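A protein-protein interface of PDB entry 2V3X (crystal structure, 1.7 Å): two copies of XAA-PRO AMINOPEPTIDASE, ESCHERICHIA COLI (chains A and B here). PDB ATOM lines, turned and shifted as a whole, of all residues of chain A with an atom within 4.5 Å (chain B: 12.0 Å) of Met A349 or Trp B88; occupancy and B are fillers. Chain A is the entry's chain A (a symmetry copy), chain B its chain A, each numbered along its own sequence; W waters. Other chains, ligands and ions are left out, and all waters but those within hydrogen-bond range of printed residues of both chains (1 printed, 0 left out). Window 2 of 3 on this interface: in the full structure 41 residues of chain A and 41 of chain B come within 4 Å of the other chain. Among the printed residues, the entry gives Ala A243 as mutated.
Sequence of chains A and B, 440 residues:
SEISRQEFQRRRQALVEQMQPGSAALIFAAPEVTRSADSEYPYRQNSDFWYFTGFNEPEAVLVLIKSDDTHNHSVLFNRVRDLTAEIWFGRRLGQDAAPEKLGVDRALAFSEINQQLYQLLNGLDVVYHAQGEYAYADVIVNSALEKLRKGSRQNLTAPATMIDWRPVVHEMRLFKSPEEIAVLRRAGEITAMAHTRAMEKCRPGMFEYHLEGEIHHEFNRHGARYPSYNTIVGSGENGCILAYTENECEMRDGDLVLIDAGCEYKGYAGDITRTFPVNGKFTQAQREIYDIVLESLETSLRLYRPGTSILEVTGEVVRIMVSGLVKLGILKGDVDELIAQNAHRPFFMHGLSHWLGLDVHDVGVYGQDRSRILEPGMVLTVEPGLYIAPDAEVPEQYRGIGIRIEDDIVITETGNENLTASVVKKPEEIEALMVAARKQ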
ATOM      1  N   ILE A 241       6.192  -5.634  22.815  1.00  0.00           N
ATOM      2  CA  ILE A 241       6.773  -4.476  23.494  1.00  0.00           C
ATOM      3  C   ILE A 241       6.136  -4.404  24.879  1.00  0.00           C
ATOM      4  O   ILE A 241       4.905  -4.263  25.018  1.00  0.00           O
ATOM      5  CB  ILE A 241       6.487  -3.178  22.703  1.00  0.00           C
ATOM      6  CG1 ILE A 241       7.112  -3.271  21.317  1.00  0.00           C
ATOM      7  CG2 ILE A 241       7.027  -1.946  23.471  1.00  0.00           C
ATOM      8  CD1 ILE A 241       6.716  -2.122  20.398  1.00  0.00           C
ATOM      9  N   LEU A 242       6.955  -4.550  25.926  1.00  0.00           N
ATOM     10  CA  LEU A 242       6.435  -4.827  27.268  1.00  0.00           C
ATOM     11  C   LEU A 242       5.509  -3.755  27.888  1.00  0.00           C
ATOM     12  O   LEU A 242       4.493  -4.077  28.525  1.00  0.00           O
ATOM     13  CB  LEU A 242       7.600  -5.116  28.232  1.00  0.00           C
ATOM     14  CG  LEU A 242       8.407  -6.366  27.865  1.00  0.00           C
ATOM     15  CD1 LEU A 242       9.500  -6.612  28.916  1.00  0.00           C
ATOM     16  CD2 LEU A 242       7.506  -7.614  27.736  1.00  0.00           C
ATOM     17  N   ALA A 243       5.881  -2.507  27.721  1.00  0.00           N
ATOM     18  CA  ALA A 243       5.090  -1.368  28.213  1.00  0.00           C
ATOM     19  C   ALA A 243       4.725  -0.457  27.035  1.00  0.00           C
ATOM     20  O   ALA A 243       4.899   0.763  27.086  1.00  0.00           O
ATOM     21  CB  ALA A 243       5.885  -0.600  29.289  1.00  0.00           C
ATOM     22  N   ARG A 345      15.401 -16.754  28.237  1.00  0.00           N
ATOM     23  CA  ARG A 345      15.485 -15.288  28.405  1.00  0.00           C
ATOM     24  C   ARG A 345      15.179 -14.435  27.173  1.00  0.00           C
ATOM     25  O   ARG A 345      14.684 -13.312  27.309  1.00  0.00           O
ATOM     26  CB  ARG A 345      16.836 -14.879  29.000  1.00  0.00           C
ATOM     27  CG  ARG A 345      16.907 -15.105  30.489  1.00  0.00           C
ATOM     28  CD  ARG A 345      18.204 -14.578  31.065  1.00  0.00           C
ATOM     29  NE  ARG A 345      18.201 -14.627  32.527  1.00  0.00           N
ATOM     30  CZ  ARG A 345      19.287 -14.557  33.291  1.00  0.00           C
ATOM     31  NH1 ARG A 345      20.498 -14.441  32.746  1.00  0.00           N
ATOM     32  NH2 ARG A 345      19.164 -14.607  34.613  1.00  0.00           N
ATOM     33  N   PRO A 346      15.471 -14.943  25.963  1.00  0.00           N
ATOM     34  CA  PRO A 346      15.031 -14.177  24.798  1.00  0.00           C
ATOM     35  C   PRO A 346      13.516 -14.047  24.659  1.00  0.00           C
ATOM     36  O   PRO A 346      13.052 -13.159  23.938  1.00  0.00           O
ATOM     37  CB  PRO A 346      15.579 -14.976  23.615  1.00  0.00           C
ATOM     38  CG  PRO A 346      16.652 -15.820  24.179  1.00  0.00           C
ATOM     39  CD  PRO A 346      16.250 -16.131  25.568  1.00  0.00           C
ATOM     40  N   PHE A 347      12.759 -14.911  25.337  1.00  0.00           N
ATOM     41  CA  PHE A 347      11.308 -14.972  25.201  1.00  0.00           C
ATOM     42  C   PHE A 347      10.567 -14.563  26.472  1.00  0.00           C
ATOM     43  O   PHE A 347       9.422 -14.169  26.404  1.00  0.00           O
ATOM     44  CB  PHE A 347      10.904 -16.399  24.804  1.00  0.00           C
ATOM     45  CG  PHE A 347      11.640 -16.905  23.595  1.00  0.00           C
ATOM     46  CD1 PHE A 347      11.439 -16.301  22.352  1.00  0.00           C
ATOM     47  CD2 PHE A 347      12.570 -17.921  23.698  1.00  0.00           C
ATOM     48  CE1 PHE A 347      12.132 -16.737  21.232  1.00  0.00           C
ATOM     49  CE2 PHE A 347      13.265 -18.360  22.583  1.00  0.00           C
ATOM     50  CZ  PHE A 347      13.045 -17.770  21.353  1.00  0.00           C
ATOM     51  N   PHE A 348      11.215 -14.693  27.626  1.00  0.00           N
ATOM     52  CA  PHE A 348      10.651 -14.241  28.901  1.00  0.00           C
ATOM     53  C   PHE A 348      11.751 -13.488  29.631  1.00  0.00           C
ATOM     54  O   PHE A 348      12.632 -14.096  30.253  1.00  0.00           O
ATOM     55  CB  PHE A 348      10.165 -15.428  29.708  1.00  0.00           C
ATOM     56  CG  PHE A 348       9.701 -15.100  31.117  1.00  0.00           C
ATOM     57  CD1 PHE A 348       8.765 -14.108  31.357  1.00  0.00           C
ATOM     58  CD2 PHE A 348      10.176 -15.840  32.205  1.00  0.00           C
ATOM     59  CE1 PHE A 348       8.315 -13.853  32.653  1.00  0.00           C
ATOM     60  CE2 PHE A 348       9.747 -15.581  33.493  1.00  0.00           C
ATOM     61  CZ  PHE A 348       8.810 -14.599  33.720  1.00  0.00           C
ATOM     62  N   MET A 349      11.731 -12.172  29.483  1.00  0.00           N
ATOM     63  CA  MET A 349      12.875 -11.350  29.863  1.00  0.00           C
ATOM     64  C   MET A 349      12.634 -10.459  31.056  1.00  0.00           C
ATOM     65  O   MET A 349      13.496  -9.618  31.383  1.00  0.00           O
ATOM     66  CB  MET A 349      13.343 -10.504  28.676  1.00  0.00           C
ATOM     67  CG  MET A 349      12.374  -9.446  28.184  1.00  0.00           C
ATOM     68  SD  MET A 349      10.901 -10.107  27.377  1.00  0.00           S
ATOM     69  CE  MET A 349      11.560 -10.976  25.953  1.00  0.00           C
ATOM     70  N   HIS A 350      11.488 -10.614  31.703  1.00  0.00           N
ATOM     71  CA  HIS A 350      11.160  -9.826  32.880  1.00  0.00           C
ATOM     72  C   HIS A 350      10.884 -10.748  34.076  1.00  0.00           C
ATOM     73  O   HIS A 350      10.969 -11.978  33.971  1.00  0.00           O
ATOM     74  CB  HIS A 350      10.000  -8.866  32.607  1.00  0.00           C
ATOM     75  CG  HIS A 350       8.723  -9.530  32.183  1.00  0.00           C
ATOM     76  ND1 HIS A 350       7.865 -10.116  33.090  1.00  0.00           N
ATOM     77  CD2 HIS A 350       8.130  -9.646  30.967  1.00  0.00           C
ATOM     78  CE1 HIS A 350       6.804 -10.581  32.444  1.00  0.00           C
ATOM     79  NE2 HIS A 350       6.942 -10.315  31.155  1.00  0.00           N
ATOM     80  N   TYR A 387       7.207 -13.784  24.582  1.00  0.00           N
ATOM     81  CA  TYR A 387       7.212 -12.773  23.520  1.00  0.00           C
ATOM     82  C   TYR A 387       8.154 -13.262  22.454  1.00  0.00           C
ATOM     83  O   TYR A 387       9.353 -13.321  22.687  1.00  0.00           O
ATOM     84  CB  TYR A 387       7.648 -11.413  24.080  1.00  0.00           C
ATOM     85  CG  TYR A 387       7.000 -11.114  25.423  1.00  0.00           C
ATOM     86  CD1 TYR A 387       7.630 -11.469  26.622  1.00  0.00           C
ATOM     87  CD2 TYR A 387       5.747 -10.545  25.509  1.00  0.00           C
ATOM     88  CE1 TYR A 387       7.044 -11.215  27.850  1.00  0.00           C
ATOM     89  CE2 TYR A 387       5.149 -10.300  26.737  1.00  0.00           C
ATOM     90  CZ  TYR A 387       5.793 -10.663  27.916  1.00  0.00           C
ATOM     91  OH  TYR A 387       5.224 -10.405  29.143  1.00  0.00           O
ATOM     92  N   GLU B  32      10.069  14.035  30.308  1.00  0.00           N
ATOM     93  CA  GLU B  32       9.120  13.109  30.929  1.00  0.00           C
ATOM     94  C   GLU B  32       8.898  13.553  32.381  1.00  0.00           C
ATOM     95  O   GLU B  32       9.789  14.150  32.998  1.00  0.00           O
ATOM     96  CB  GLU B  32       9.663  11.694  30.869  1.00  0.00           C
ATOM     97  CG  GLU B  32       9.803  11.180  29.453  1.00  0.00           C
ATOM     98  CD  GLU B  32      10.144   9.702  29.373  1.00  0.00           C
ATOM     99  OE1 GLU B  32      11.342   9.354  29.407  1.00  0.00           O
ATOM    100  OE2 GLU B  32       9.198   8.895  29.249  1.00  0.00           O
ATOM    101  N   ASP B  38       8.312   5.128  40.172  1.00  0.00           N
ATOM    102  CA  ASP B  38       8.852   4.865  38.834  1.00  0.00           C
ATOM    103  C   ASP B  38       7.819   4.987  37.710  1.00  0.00           C
ATOM    104  O   ASP B  38       8.144   4.730  36.547  1.00  0.00           O
ATOM    105  CB  ASP B  38       9.589   3.513  38.772  1.00  0.00           C
ATOM    106  CG  ASP B  38       8.676   2.307  38.960  1.00  0.00           C
ATOM    107  OD1 ASP B  38       7.679   2.433  39.708  1.00  0.00           O
ATOM    108  OD2 ASP B  38       8.988   1.219  38.392  1.00  0.00           O
ATOM    109  N   GLU B  40       5.358   7.216  35.210  1.00  0.00           N
ATOM    110  CA  GLU B  40       5.285   8.542  34.619  1.00  0.00           C
ATOM    111  C   GLU B  40       3.880   8.857  34.115  1.00  0.00           C
ATOM    112  O   GLU B  40       3.080   7.957  33.822  1.00  0.00           O
ATOM    113  CB  GLU B  40       6.292   8.632  33.474  1.00  0.00           C
ATOM    114  CG  GLU B  40       7.726   8.397  33.927  1.00  0.00           C
ATOM    115  CD  GLU B  40       8.680   8.121  32.780  1.00  0.00           C
ATOM    116  OE1 GLU B  40       8.291   8.320  31.603  1.00  0.00           O
ATOM    117  OE2 GLU B  40       9.815   7.700  33.073  1.00  0.00           O
ATOM    118  N   ARG B  79      16.641  10.356  20.444  1.00  0.00           N
ATOM    119  CA  ARG B  79      17.122   9.098  20.993  1.00  0.00           C
ATOM    120  C   ARG B  79      17.519   8.084  19.930  1.00  0.00           C
ATOM    121  O   ARG B  79      16.826   7.892  18.939  1.00  0.00           O
ATOM    122  CB  ARG B  79      16.074   8.469  21.881  1.00  0.00           C
ATOM    123  CG  ARG B  79      15.847   9.222  23.168  1.00  0.00           C
ATOM    124  CD  ARG B  79      14.525   8.770  23.772  1.00  0.00           C
ATOM    125  NE  ARG B  79      14.538   8.985  25.204  1.00  0.00           N
ATOM    126  CZ  ARG B  79      13.543   8.645  26.016  1.00  0.00           C
ATOM    127  NH1 ARG B  79      12.451   8.076  25.526  1.00  0.00           N
ATOM    128  NH2 ARG B  79      13.650   8.877  27.323  1.00  0.00           N
ATOM    129  N   VAL B  80      18.635   7.415  20.181  1.00  0.00           N
ATOM    130  CA  VAL B  80      19.109   6.359  19.287  1.00  0.00           C
ATOM    131  C   VAL B  80      18.188   5.142  19.323  1.00  0.00           C
ATOM    132  O   VAL B  80      17.535   4.865  20.337  1.00  0.00           O
ATOM    133  CB  VAL B  80      20.548   5.934  19.679  1.00  0.00           C
ATOM    134  CG1 VAL B  80      20.544   5.216  21.035  1.00  0.00           C
ATOM    135  CG2 VAL B  80      21.178   5.061  18.588  1.00  0.00           C
ATOM    136  N   ARG B  81      18.142   4.404  18.214  1.00  0.00           N
ATOM    137  CA  ARG B  81      17.640   3.008  18.242  1.00  0.00           C
ATOM    138  C   ARG B  81      18.394   2.192  19.286  1.00  0.00           C
ATOM    139  O   ARG B  81      19.640   2.231  19.383  1.00  0.00           O
ATOM    140  CB  ARG B  81      17.828   2.301  16.896  1.00  0.00           C
ATOM    141  CG  ARG B  81      17.134   2.954  15.686  1.00  0.00           C
ATOM    142  CD  ARG B  81      15.710   3.322  15.946  1.00  0.00           C
ATOM    143  NE  ARG B  81      14.871   2.162  16.226  1.00  0.00           N
ATOM    144  CZ  ARG B  81      14.251   1.422  15.309  1.00  0.00           C
ATOM    145  NH1 ARG B  81      14.418   1.645  14.012  1.00  0.00           N
ATOM    146  NH2 ARG B  81      13.486   0.407  15.697  1.00  0.00           N
ATOM    147  N   ASP B  82      17.648   1.431  20.063  1.00  0.00           N
ATOM    148  CA  ASP B  82      18.232   0.596  21.114  1.00  0.00           C
ATOM    149  C   ASP B  82      17.271  -0.554  21.357  1.00  0.00           C
ATOM    150  O   ASP B  82      16.181  -0.347  21.900  1.00  0.00           O
ATOM    151  CB  ASP B  82      18.418   1.397  22.406  1.00  0.00           C
ATOM    152  CG  ASP B  82      19.083   0.590  23.506  1.00  0.00           C
ATOM    153  OD1 ASP B  82      18.385  -0.169  24.215  1.00  0.00           O
ATOM    154  OD2 ASP B  82      20.319   0.709  23.657  1.00  0.00           O
ATOM    155  N   LEU B  83      17.687  -1.757  20.979  1.00  0.00           N
ATOM    156  CA  LEU B  83      16.796  -2.915  21.022  1.00  0.00           C
ATOM    157  C   LEU B  83      16.190  -3.116  22.397  1.00  0.00           C
ATOM    158  O   LEU B  83      14.973  -3.297  22.507  1.00  0.00           O
ATOM    159  CB  LEU B  83      17.508  -4.196  20.566  1.00  0.00           C
ATOM    160  CG  LEU B  83      16.581  -5.403  20.365  1.00  0.00           C
ATOM    161  CD1 LEU B  83      15.343  -5.015  19.544  1.00  0.00           C
ATOM    162  CD2 LEU B  83      17.318  -6.586  19.723  1.00  0.00           C
ATOM    163  N   THR B  84      17.012  -3.070  23.445  1.00  0.00           N
ATOM    164  CA  THR B  84      16.503  -3.364  24.799  1.00  0.00           C
ATOM    165  C   THR B  84      15.535  -2.301  25.308  1.00  0.00           C
ATOM    166  O   THR B  84      14.473  -2.618  25.841  1.00  0.00           O
ATOM    167  CB  THR B  84      17.641  -3.535  25.821  1.00  0.00           C
ATOM    168  OG1 THR B  84      18.449  -4.641  25.422  1.00  0.00           O
ATOM    169  CG2 THR B  84      17.074  -3.822  27.223  1.00  0.00           C
ATOM    170  N   ALA B  85      15.902  -1.036  25.142  1.00  0.00           N
ATOM    171  CA  ALA B  85      15.029   0.062  25.558  1.00  0.00           C
ATOM    172  C   ALA B  85      13.710   0.009  24.805  1.00  0.00           C
ATOM    173  O   ALA B  85      12.652   0.338  25.356  1.00  0.00           O
ATOM    174  CB  ALA B  85      15.719   1.406  25.336  1.00  0.00           C
ATOM    175  N   GLU B  86      13.775  -0.409  23.540  1.00  0.00           N
ATOM    176  CA  GLU B  86      12.579  -0.470  22.718  1.00  0.00           C
ATOM    177  C   GLU B  86      11.684  -1.665  23.051  1.00  0.00           C
ATOM    178  O   GLU B  86      10.481  -1.484  23.109  1.00  0.00           O
ATOM    179  CB  GLU B  86      12.915  -0.379  21.227  1.00  0.00           C
ATOM    180  CG  GLU B  86      13.432   1.011  20.866  1.00  0.00           C
ATOM    181  CD  GLU B  86      13.705   1.171  19.390  1.00  0.00           C
ATOM    182  OE1 GLU B  86      12.765   1.011  18.571  1.00  0.00           O
ATOM    183  OE2 GLU B  86      14.871   1.469  19.061  1.00  0.00           O
ATOM    184  N   ILE B  87      12.245  -2.847  23.277  1.00  0.00           N
ATOM    185  CA  ILE B  87      11.448  -3.999  23.786  1.00  0.00           C
ATOM    186  C   ILE B  87      10.685  -3.627  25.063  1.00  0.00           C
ATOM    187  O   ILE B  87       9.561  -4.076  25.282  1.00  0.00           O
ATOM    188  CB  ILE B  87      12.316  -5.249  24.077  1.00  0.00           C
ATOM    189  CG1 ILE B  87      12.819  -5.866  22.773  1.00  0.00           C
ATOM    190  CG2 ILE B  87      11.540  -6.307  24.892  1.00  0.00           C
ATOM    191  CD1 ILE B  87      13.904  -6.904  22.986  1.00  0.00           C
ATOM    192  N   TRP B  88      11.298  -2.825  25.918  1.00  0.00           N
ATOM    193  CA  TRP B  88      10.656  -2.460  27.186  1.00  0.00           C
ATOM    194  C   TRP B  88       9.639  -1.339  27.069  1.00  0.00           C
ATOM    195  O   TRP B  88       8.500  -1.478  27.536  1.00  0.00           O
ATOM    196  CB  TRP B  88      11.721  -2.123  28.234  1.00  0.00           C
ATOM    197  CG  TRP B  88      12.334  -3.380  28.824  1.00  0.00           C
ATOM    198  CD1 TRP B  88      13.332  -4.141  28.283  1.00  0.00           C
ATOM    199  CD2 TRP B  88      11.954  -4.035  30.048  1.00  0.00           C
ATOM    200  NE1 TRP B  88      13.595  -5.225  29.093  1.00  0.00           N
ATOM    201  CE2 TRP B  88      12.765  -5.180  30.181  1.00  0.00           C
ATOM    202  CE3 TRP B  88      11.003  -3.765  31.039  1.00  0.00           C
ATOM    203  CZ2 TRP B  88      12.666  -6.056  31.277  1.00  0.00           C
ATOM    204  CZ3 TRP B  88      10.904  -4.643  32.130  1.00  0.00           C
ATOM    205  CH2 TRP B  88      11.737  -5.761  32.235  1.00  0.00           C
ATOM    206  N   PHE B  89      10.041  -0.234  26.439  1.00  0.00           N
ATOM    207  CA  PHE B  89       9.335   1.047  26.596  1.00  0.00           C
ATOM    208  C   PHE B  89       8.713   1.605  25.332  1.00  0.00           C
ATOM    209  O   PHE B  89       7.946   2.582  25.394  1.00  0.00           O
ATOM    210  CB  PHE B  89      10.279   2.083  27.207  1.00  0.00           C
ATOM    211  CG  PHE B  89      10.843   1.650  28.528  1.00  0.00           C
ATOM    212  CD1 PHE B  89       9.988   1.349  29.590  1.00  0.00           C
ATOM    213  CD2 PHE B  89      12.207   1.495  28.705  1.00  0.00           C
ATOM    214  CE1 PHE B  89      10.492   0.921  30.805  1.00  0.00           C
ATOM    215  CE2 PHE B  89      12.720   1.074  29.923  1.00  0.00           C
ATOM    216  CZ  PHE B  89      11.864   0.788  30.975  1.00  0.00           C
ATOM    217  N   GLY B  90       9.034   1.007  24.190  1.00  0.00           N
ATOM    218  CA  GLY B  90       8.413   1.405  22.954  1.00  0.00           C
ATOM    219  C   GLY B  90       9.426   1.802  21.908  1.00  0.00           C
ATOM    220  O   GLY B  90      10.607   2.032  22.195  1.00  0.00           O
ATOM    221  N   ARG B  91       8.933   1.902  20.691  1.00  0.00           N
ATOM    222  CA  ARG B  91       9.796   2.103  19.560  1.00  0.00           C
ATOM    223  C   ARG B  91      10.295   3.530  19.569  1.00  0.00           C
ATOM    224  O   ARG B  91       9.661   4.423  20.154  1.00  0.00           O
ATOM    225  CB  ARG B  91       9.045   1.824  18.274  1.00  0.00           C
ATOM    226  CG  ARG B  91       8.494   0.427  18.191  1.00  0.00           C
ATOM    227  CD  ARG B  91       7.895   0.226  16.836  1.00  0.00           C
ATOM    228  NE  ARG B  91       7.379  -1.118  16.703  1.00  0.00           N
ATOM    229  CZ  ARG B  91       6.164  -1.512  17.094  1.00  0.00           C
ATOM    230  NH1 ARG B  91       5.302  -0.647  17.630  1.00  0.00           N
ATOM    231  NH2 ARG B  91       5.820  -2.776  16.923  1.00  0.00           N
ATOM    232  N   ARG B  92      11.457   3.720  18.956  1.00  0.00           N
ATOM    233  CA  ARG B  92      12.071   5.035  18.802  1.00  0.00           C
ATOM    234  C   ARG B  92      12.312   5.257  17.332  1.00  0.00           C
ATOM    235  O   ARG B  92      12.599   4.311  16.584  1.00  0.00           O
ATOM    236  CB  ARG B  92      13.412   5.090  19.512  1.00  0.00           C
ATOM    237  CG  ARG B  92      13.328   4.975  20.991  1.00  0.00           C
ATOM    238  CD  ARG B  92      14.674   4.613  21.530  1.00  0.00           C
ATOM    239  NE  ARG B  92      14.692   4.675  22.985  1.00  0.00           N
ATOM    240  CZ  ARG B  92      15.787   4.868  23.715  1.00  0.00           C
ATOM    241  NH1 ARG B  92      16.986   5.055  23.150  1.00  0.00           N
ATOM    242  NH2 ARG B  92      15.669   4.898  25.035  1.00  0.00           N
HETATM  243  O   HOH W   1       5.183   3.124  24.546  1.00  0.00           O
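No position is printed for both chains. Of the 10 pairs that touch across the chains among the printed residues, none has its exchanged pair printed and touching as well.
O of Ile B87 is in hydrogen-bond range of N of Leu A242 (2.7 Å). O of Trp B88 is in hydrogen-bond range of N of Ala A243, 2.8 Å away.
Hydrophobic or aromatic side chains of chain A that line the printed part of chain B: Ile A241, Leu A242, Ala A243 and His A350. Along chain A the printed residues that touch a printed residue of chain B span positions 241 to 350. Among the printed residues, 10 pairs touch across the chains. Among the printed residues, no Asp or Glu carboxylate lies within 4 Å of a Lys or Arg side-chain nitrogen of the other chain.
Of the printed residues of chain A, Trp B88 touches Leu A242 (3.7 Å), Ala A243 (2.8 Å), Met A349 (3.7 Å) and His A350 (3.6 Å). Of the printed residues of chain B, Ile A241 touches Glu B86, Ile B87, Gly B90 and Arg B91. Ala A243 touches just these residues of chain B: Trp B88 and Phe B89. No residue of chain B comes within 4 Å of Pro A346. No residue of chain B comes within 4 Å of Phe A348. No residue of chain B comes within 4 Å of Tyr A387. Of the printed residues of chain A, Arg B91 touches Ile A241 (3.4 Å). Of the printed residues of chain A, Gly B90 touches Ile A241. Printed residues of chain A within 4 Å of Ile B87: Ile A241 and Leu A242. Val B80 touches none of the printed residues of chain A. Arg A345 touches none of the printed residues of chain B. The nearest residue of chain B that does not touch Met A349 is Ile B87 (4.6 Å).
Glu B86 touches Ile A241. Ile A241 touches Ile B87 (CA to O, 3.3 Å). Gly B90 touches Ile A241. Arg B91 touches Ile A241. Trp B88 touches Leu A242 (CD2 to CD1, 3.7 Å). O of Phe B89 touches O of Ala A243, at 3.9 Å. Trp B88 touches Met A349 (CZ2 to O, 3.7 Å). Trp B88 touches His A350 (CH2 to CB, 3.6 Å).
Water W1 bridges O of Phe B89 (2.9 Å) and O of Ala A243 (3.5 Å).
OE2 of Glu B86 is in salt-bridge range of NE of Arg B81 (2.9 Å). N of Asp B82 sits at hydrogen-bond distance from OE2 of Glu B86 (3.0 Å). OE1 of Glu B86 lies within hydrogen-bond range of N of Arg B92, 3.0 Å away. A ring nitrogen (NE2) of His A350 sits at hydrogen-bond distance from the side-chain hydroxyl (OH) of Tyr A387, at 2.6 Å.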
